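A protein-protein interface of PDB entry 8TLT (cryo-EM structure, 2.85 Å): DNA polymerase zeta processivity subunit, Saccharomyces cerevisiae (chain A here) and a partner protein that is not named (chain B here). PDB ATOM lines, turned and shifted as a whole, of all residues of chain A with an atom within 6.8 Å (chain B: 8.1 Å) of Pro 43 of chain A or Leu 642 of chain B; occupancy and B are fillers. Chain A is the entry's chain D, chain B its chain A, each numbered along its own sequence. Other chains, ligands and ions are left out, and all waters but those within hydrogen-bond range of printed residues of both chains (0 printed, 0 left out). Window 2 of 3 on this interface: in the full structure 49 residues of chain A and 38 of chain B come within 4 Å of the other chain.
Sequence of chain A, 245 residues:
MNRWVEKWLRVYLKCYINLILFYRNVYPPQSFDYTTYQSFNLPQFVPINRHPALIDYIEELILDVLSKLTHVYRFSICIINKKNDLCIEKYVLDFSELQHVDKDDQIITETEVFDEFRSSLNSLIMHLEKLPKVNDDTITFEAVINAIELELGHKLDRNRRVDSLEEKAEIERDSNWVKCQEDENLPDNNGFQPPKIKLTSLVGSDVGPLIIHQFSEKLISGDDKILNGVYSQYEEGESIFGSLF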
ATOM      1  N   PHE A  40     -13.307   9.945  -2.993  1.00  0.00           N
ATOM      2  CA  PHE A  40     -13.866  11.105  -2.301  1.00  0.00           C
ATOM      3  C   PHE A  40     -12.810  11.738  -1.404  1.00  0.00           C
ATOM      4  O   PHE A  40     -13.058  12.046  -0.238  1.00  0.00           O
ATOM      5  CB  PHE A  40     -15.099  10.717  -1.487  1.00  0.00           C
ATOM      6  CG  PHE A  40     -16.390  10.809  -2.247  1.00  0.00           C
ATOM      7  CD1 PHE A  40     -16.778   9.798  -3.106  1.00  0.00           C
ATOM      8  CD2 PHE A  40     -17.223  11.902  -2.091  1.00  0.00           C
ATOM      9  CE1 PHE A  40     -17.964   9.879  -3.798  1.00  0.00           C
ATOM     10  CE2 PHE A  40     -18.412  11.988  -2.782  1.00  0.00           C
ATOM     11  CZ  PHE A  40     -18.782  10.975  -3.637  1.00  0.00           C
ATOM     12  N   ASN A  41     -11.607  11.921  -1.947  1.00  0.00           N
ATOM     13  CA  ASN A  41     -10.446  12.421  -1.211  1.00  0.00           C
ATOM     14  C   ASN A  41     -10.022  11.467  -0.100  1.00  0.00           C
ATOM     15  O   ASN A  41      -9.305  11.864   0.821  1.00  0.00           O
ATOM     16  CB  ASN A  41     -10.700  13.819  -0.630  1.00  0.00           C
ATOM     17  CG  ASN A  41     -10.733  14.895  -1.691  1.00  0.00           C
ATOM     18  OD1 ASN A  41     -11.481  15.864  -1.584  1.00  0.00           O
ATOM     19  ND2 ASN A  41      -9.930  14.723  -2.729  1.00  0.00           N
ATOM     20  N   LEU A  42     -10.458  10.216  -0.171  1.00  0.00           N
ATOM     21  CA  LEU A  42     -10.143   9.236   0.853  1.00  0.00           C
ATOM     22  C   LEU A  42      -8.729   8.690   0.665  1.00  0.00           C
ATOM     23  O   LEU A  42      -8.241   8.583  -0.462  1.00  0.00           O
ATOM     24  CB  LEU A  42     -11.149   8.092   0.817  1.00  0.00           C
ATOM     25  CG  LEU A  42     -12.562   8.454   1.278  1.00  0.00           C
ATOM     26  CD1 LEU A  42     -13.598   7.610   0.564  1.00  0.00           C
ATOM     27  CD2 LEU A  42     -12.687   8.296   2.780  1.00  0.00           C
ATOM     28  N   PRO A  43      -8.051   8.338   1.761  1.00  0.00           N
ATOM     29  CA  PRO A  43      -6.682   7.814   1.636  1.00  0.00           C
ATOM     30  C   PRO A  43      -6.611   6.415   1.048  1.00  0.00           C
ATOM     31  O   PRO A  43      -5.510   5.966   0.705  1.00  0.00           O
ATOM     32  CB  PRO A  43      -6.170   7.833   3.080  1.00  0.00           C
ATOM     33  CG  PRO A  43      -7.401   7.728   3.914  1.00  0.00           C
ATOM     34  CD  PRO A  43      -8.470   8.469   3.166  1.00  0.00           C
ATOM     35  N   GLN A  44      -7.733   5.712   0.931  1.00  0.00           N
ATOM     36  CA  GLN A  44      -7.727   4.336   0.465  1.00  0.00           C
ATOM     37  C   GLN A  44      -7.714   4.270  -1.060  1.00  0.00           C
ATOM     38  O   GLN A  44      -8.120   5.205  -1.756  1.00  0.00           O
ATOM     39  CB  GLN A  44      -8.945   3.582   1.000  1.00  0.00           C
ATOM     40  CG  GLN A  44      -8.964   3.421   2.506  1.00  0.00           C
ATOM     41  CD  GLN A  44     -10.146   4.115   3.147  1.00  0.00           C
ATOM     42  OE1 GLN A  44     -10.611   5.146   2.663  1.00  0.00           O
ATOM     43  NE2 GLN A  44     -10.639   3.554   4.243  1.00  0.00           N
ATOM     44  N   PHE A  45      -7.235   3.141  -1.574  1.00  0.00           N
ATOM     45  CA  PHE A  45      -7.308   2.875  -3.003  1.00  0.00           C
ATOM     46  C   PHE A  45      -8.738   2.532  -3.400  1.00  0.00           C
ATOM     47  O   PHE A  45      -9.439   1.808  -2.688  1.00  0.00           O
ATOM     48  CB  PHE A  45      -6.380   1.721  -3.380  1.00  0.00           C
ATOM     49  CG  PHE A  45      -4.930   2.096  -3.435  1.00  0.00           C
ATOM     50  CD1 PHE A  45      -4.508   3.188  -4.169  1.00  0.00           C
ATOM     51  CD2 PHE A  45      -3.985   1.347  -2.758  1.00  0.00           C
ATOM     52  CE1 PHE A  45      -3.172   3.530  -4.222  1.00  0.00           C
ATOM     53  CE2 PHE A  45      -2.649   1.683  -2.807  1.00  0.00           C
ATOM     54  CZ  PHE A  45      -2.243   2.775  -3.540  1.00  0.00           C
ATOM     55  N   ARG A 118     -18.602  10.722   1.409  1.00  0.00           N
ATOM     56  CA  ARG A 118     -17.255  10.274   1.741  1.00  0.00           C
ATOM     57  C   ARG A 118     -17.260   9.362   2.963  1.00  0.00           C
ATOM     58  O   ARG A 118     -16.586   8.325   2.978  1.00  0.00           O
ATOM     59  CB  ARG A 118     -16.355  11.492   1.962  1.00  0.00           C
ATOM     60  CG  ARG A 118     -14.957  11.196   2.471  1.00  0.00           C
ATOM     61  CD  ARG A 118     -14.275  12.483   2.917  1.00  0.00           C
ATOM     62  NE  ARG A 118     -13.020  12.246   3.620  1.00  0.00           N
ATOM     63  CZ  ARG A 118     -11.839  12.130   3.028  1.00  0.00           C
ATOM     64  N   ASN A 122     -16.284   5.421   3.045  1.00  0.00           N
ATOM     65  CA  ASN A 122     -15.274   4.908   3.966  1.00  0.00           C
ATOM     66  C   ASN A 122     -15.810   3.726   4.761  1.00  0.00           C
ATOM     67  O   ASN A 122     -15.113   2.718   4.937  1.00  0.00           O
ATOM     68  CB  ASN A 122     -14.805   6.014   4.909  1.00  0.00           C
ATOM     69  CG  ASN A 122     -13.542   5.641   5.657  1.00  0.00           C
ATOM     70  N   MET A 126     -14.323  -0.091   4.609  1.00  0.00           N
ATOM     71  CA  MET A 126     -13.898  -0.775   5.826  1.00  0.00           C
ATOM     72  C   MET A 126     -14.651  -2.085   6.012  1.00  0.00           C
ATOM     73  O   MET A 126     -14.059  -3.098   6.403  1.00  0.00           O
ATOM     74  CB  MET A 126     -14.094   0.138   7.036  1.00  0.00           C
ATOM     75  CG  MET A 126     -13.148   1.327   7.079  1.00  0.00           C
ATOM     76  SD  MET A 126     -11.416   0.847   7.218  1.00  0.00           S
ATOM     77  N   THR B 609       1.865   6.798  -6.612  1.00  0.00           N
ATOM     78  CA  THR B 609       0.660   6.179  -6.080  1.00  0.00           C
ATOM     79  C   THR B 609       0.068   6.953  -4.908  1.00  0.00           C
ATOM     80  O   THR B 609      -0.973   6.549  -4.382  1.00  0.00           O
ATOM     81  CB  THR B 609       0.961   4.736  -5.660  1.00  0.00           C
ATOM     82  OG1 THR B 609      -0.257   3.984  -5.621  1.00  0.00           O
ATOM     83  CG2 THR B 609       1.624   4.699  -4.291  1.00  0.00           C
ATOM     84  N   HIS B 610       0.700   8.049  -4.502  1.00  0.00           N
ATOM     85  CA  HIS B 610       0.205   8.862  -3.402  1.00  0.00           C
ATOM     86  C   HIS B 610      -1.133   9.497  -3.760  1.00  0.00           C
ATOM     87  O   HIS B 610      -1.423   9.775  -4.926  1.00  0.00           O
ATOM     88  CB  HIS B 610       1.226   9.945  -3.054  1.00  0.00           C
ATOM     89  CG  HIS B 610       0.996  10.598  -1.727  1.00  0.00           C
ATOM     90  ND1 HIS B 610       0.481  11.871  -1.604  1.00  0.00           N
ATOM     91  CD2 HIS B 610       1.225  10.163  -0.466  1.00  0.00           C
ATOM     92  CE1 HIS B 610       0.395  12.187  -0.325  1.00  0.00           C
ATOM     93  NE2 HIS B 610       0.841  11.168   0.386  1.00  0.00           N
ATOM     94  N   VAL B 611      -1.954   9.729  -2.733  1.00  0.00           N
ATOM     95  CA  VAL B 611      -3.290  10.278  -2.939  1.00  0.00           C
ATOM     96  C   VAL B 611      -3.247  11.691  -3.504  1.00  0.00           C
ATOM     97  O   VAL B 611      -4.215  12.135  -4.130  1.00  0.00           O
ATOM     98  CB  VAL B 611      -4.088  10.228  -1.616  1.00  0.00           C
ATOM     99  CG1 VAL B 611      -3.594  11.288  -0.647  1.00  0.00           C
ATOM    100  CG2 VAL B 611      -5.578  10.388  -1.879  1.00  0.00           C
ATOM    101  N   ARG B 614      -3.137  11.239  -7.332  1.00  0.00           N
ATOM    102  CA  ARG B 614      -4.164  10.384  -7.907  1.00  0.00           C
ATOM    103  C   ARG B 614      -5.331  11.232  -8.397  1.00  0.00           C
ATOM    104  O   ARG B 614      -5.824  12.101  -7.673  1.00  0.00           O
ATOM    105  CB  ARG B 614      -4.640   9.359  -6.881  1.00  0.00           C
ATOM    106  CG  ARG B 614      -3.761   8.126  -6.786  1.00  0.00           C
ATOM    107  CD  ARG B 614      -4.475   6.999  -6.061  1.00  0.00           C
ATOM    108  NE  ARG B 614      -4.002   6.835  -4.693  1.00  0.00           N
ATOM    109  CZ  ARG B 614      -4.792   6.753  -3.632  1.00  0.00           C
ATOM    110  NH1 ARG B 614      -6.107   6.821  -3.743  1.00  0.00           N
ATOM    111  NH2 ARG B 614      -4.247   6.597  -2.430  1.00  0.00           N
ATOM    112  N   LYS B 639     -13.178  11.123  12.699  1.00  0.00           N
ATOM    113  CA  LYS B 639     -12.630   9.807  12.992  1.00  0.00           C
ATOM    114  C   LYS B 639     -11.367   9.586  12.167  1.00  0.00           C
ATOM    115  O   LYS B 639     -11.240  10.093  11.052  1.00  0.00           O
ATOM    116  CB  LYS B 639     -13.656   8.712  12.690  1.00  0.00           C
ATOM    117  CG  LYS B 639     -13.310   7.348  13.246  1.00  0.00           C
ATOM    118  CD  LYS B 639     -14.487   6.388  13.153  1.00  0.00           C
ATOM    119  CE  LYS B 639     -15.529   6.837  12.142  1.00  0.00           C
ATOM    120  NZ  LYS B 639     -16.724   5.949  12.154  1.00  0.00           N
ATOM    121  N   TYR B 640     -10.434   8.803  12.711  1.00  0.00           N
ATOM    122  CA  TYR B 640      -9.087   8.755  12.151  1.00  0.00           C
ATOM    123  C   TYR B 640      -8.954   7.813  10.958  1.00  0.00           C
ATOM    124  O   TYR B 640      -7.887   7.782  10.336  1.00  0.00           O
ATOM    125  CB  TYR B 640      -8.084   8.381  13.249  1.00  0.00           C
ATOM    126  CG  TYR B 640      -6.653   8.234  12.778  1.00  0.00           C
ATOM    127  CD1 TYR B 640      -5.925   9.336  12.355  1.00  0.00           C
ATOM    128  CD2 TYR B 640      -6.027   6.999  12.778  1.00  0.00           C
ATOM    129  CE1 TYR B 640      -4.621   9.208  11.929  1.00  0.00           C
ATOM    130  CE2 TYR B 640      -4.722   6.864  12.356  1.00  0.00           C
ATOM    131  CZ  TYR B 640      -4.024   7.971  11.933  1.00  0.00           C
ATOM    132  OH  TYR B 640      -2.723   7.835  11.513  1.00  0.00           O
ATOM    133  N   ALA B 641      -9.995   7.049  10.624  1.00  0.00           N
ATOM    134  CA  ALA B 641     -10.032   6.280   9.382  1.00  0.00           C
ATOM    135  C   ALA B 641      -9.011   5.147   9.375  1.00  0.00           C
ATOM    136  O   ALA B 641      -9.388   3.980   9.523  1.00  0.00           O
ATOM    137  CB  ALA B 641      -9.826   7.190   8.165  1.00  0.00           C
ATOM    138  N   LEU B 642      -7.734   5.478   9.167  1.00  0.00           N
ATOM    139  CA  LEU B 642      -6.662   4.491   9.056  1.00  0.00           C
ATOM    140  C   LEU B 642      -6.776   3.405  10.118  1.00  0.00           C
ATOM    141  O   LEU B 642      -6.893   3.693  11.311  1.00  0.00           O
ATOM    142  CB  LEU B 642      -5.294   5.173   9.167  1.00  0.00           C
ATOM    143  CG  LEU B 642      -4.658   5.829   7.938  1.00  0.00           C
ATOM    144  CD1 LEU B 642      -5.663   6.614   7.115  1.00  0.00           C
ATOM    145  CD2 LEU B 642      -3.492   6.712   8.349  1.00  0.00           C
ATOM    146  N   LYS B 643      -6.741   2.152   9.670  1.00  0.00           N
ATOM    147  CA  LYS B 643      -6.907   0.977  10.515  1.00  0.00           C
ATOM    148  C   LYS B 643      -5.581   0.589  11.165  1.00  0.00           C
ATOM    149  O   LYS B 643      -4.540   0.577  10.501  1.00  0.00           O
ATOM    150  CB  LYS B 643      -7.442  -0.200   9.702  1.00  0.00           C
ATOM    151  CG  LYS B 643      -6.752  -0.405   8.366  1.00  0.00           C
ATOM    152  CD  LYS B 643      -7.235  -1.675   7.687  1.00  0.00           C
ATOM    153  N   PRO B 644      -5.605   0.277  12.457  1.00  0.00           N
ATOM    154  CA  PRO B 644      -4.385  -0.134  13.150  1.00  0.00           C
ATOM    155  C   PRO B 644      -4.034  -1.573  12.819  1.00  0.00           C
ATOM    156  O   PRO B 644      -4.836  -2.290  12.204  1.00  0.00           O
ATOM    157  CB  PRO B 644      -4.757   0.023  14.630  1.00  0.00           C
ATOM    158  CG  PRO B 644      -6.222  -0.178  14.661  1.00  0.00           C
ATOM    159  CD  PRO B 644      -6.758   0.368  13.369  1.00  0.00           C
ATOM    160  N   PRO B 645      -2.839  -2.031  13.197  1.00  0.00           N
ATOM    161  CA  PRO B 645      -2.515  -3.451  13.030  1.00  0.00           C
ATOM    162  C   PRO B 645      -3.466  -4.329  13.827  1.00  0.00           C
ATOM    163  O   PRO B 645      -3.980  -3.936  14.876  1.00  0.00           O
ATOM    164  CB  PRO B 645      -1.080  -3.554  13.558  1.00  0.00           C
ATOM    165  CG  PRO B 645      -0.532  -2.179  13.435  1.00  0.00           C
ATOM    166  CD  PRO B 645      -1.682  -1.253  13.669  1.00  0.00           C
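Val 611 of chain B touches Leu 42 of chain A. CD1 of Leu 642 of chain B touches CG of Pro 43 of chain A, 3.8 Å away. CZ of Phe 45 of chain A touches OG1 of Thr 609 of chain B, at 3.1 Å. Phe 45 of chain A touches Arg 614 of chain B.
Of the 11 printed residues of chain B, 4 touch a printed residue of chain A. Printed residues of chain B that touch a printed residue of chain A: Thr 609, Val 611, Arg 614 and Leu 642. Hydrophobic or aromatic side chains of chain A that line the printed part of chain B: Pro 43 and Phe 45. Among the printed residues, 6 pairs touch across the chains. Among the printed residues, no Asp or Glu carboxylate lies within 4 Å of a Lys or Arg side-chain nitrogen of the other chain.
NE of Arg 614 of chain B is in hydrogen-bond range of O of Thr 609 of chain B (3.1 Å).
NH2 of Arg 614 of chain B is in hydrogen-bond range of O of Pro 43 of chain A, at 3.4 Å. NH1 of Arg 614 of chain B is in hydrogen-bond range of O of Gln 44 of chain A (3.3 Å).
Pro 43 of chain A touches just these residues of chain B: Arg 614 (3.4 Å) and Leu 642 (3.8 Å). Leu 642 of chain B touches just one residue of chain A: Pro 43 (3.8 Å). Printed residues of chain A within 4 Å of Val 611 of chain B: Leu 42 (3.5 Å). Of the printed residues of chain B, Phe 45 of chain A touches Thr 609 (3.1 Å) and Arg 614 (3.4 Å). Of the printed residues of chain B, Gln 44 of chain A touches Arg 614. Of the printed residues of chain A, Thr 609 of chain B touches Phe 45. The nearest residue of chain B that does not touch Pro 43 of chain A is Val 611 of chain B (4.5 Å). The nearest printed residue of chain A that does not touch Leu 642 of chain B is Gln 44 of chain A (6.0 Å).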
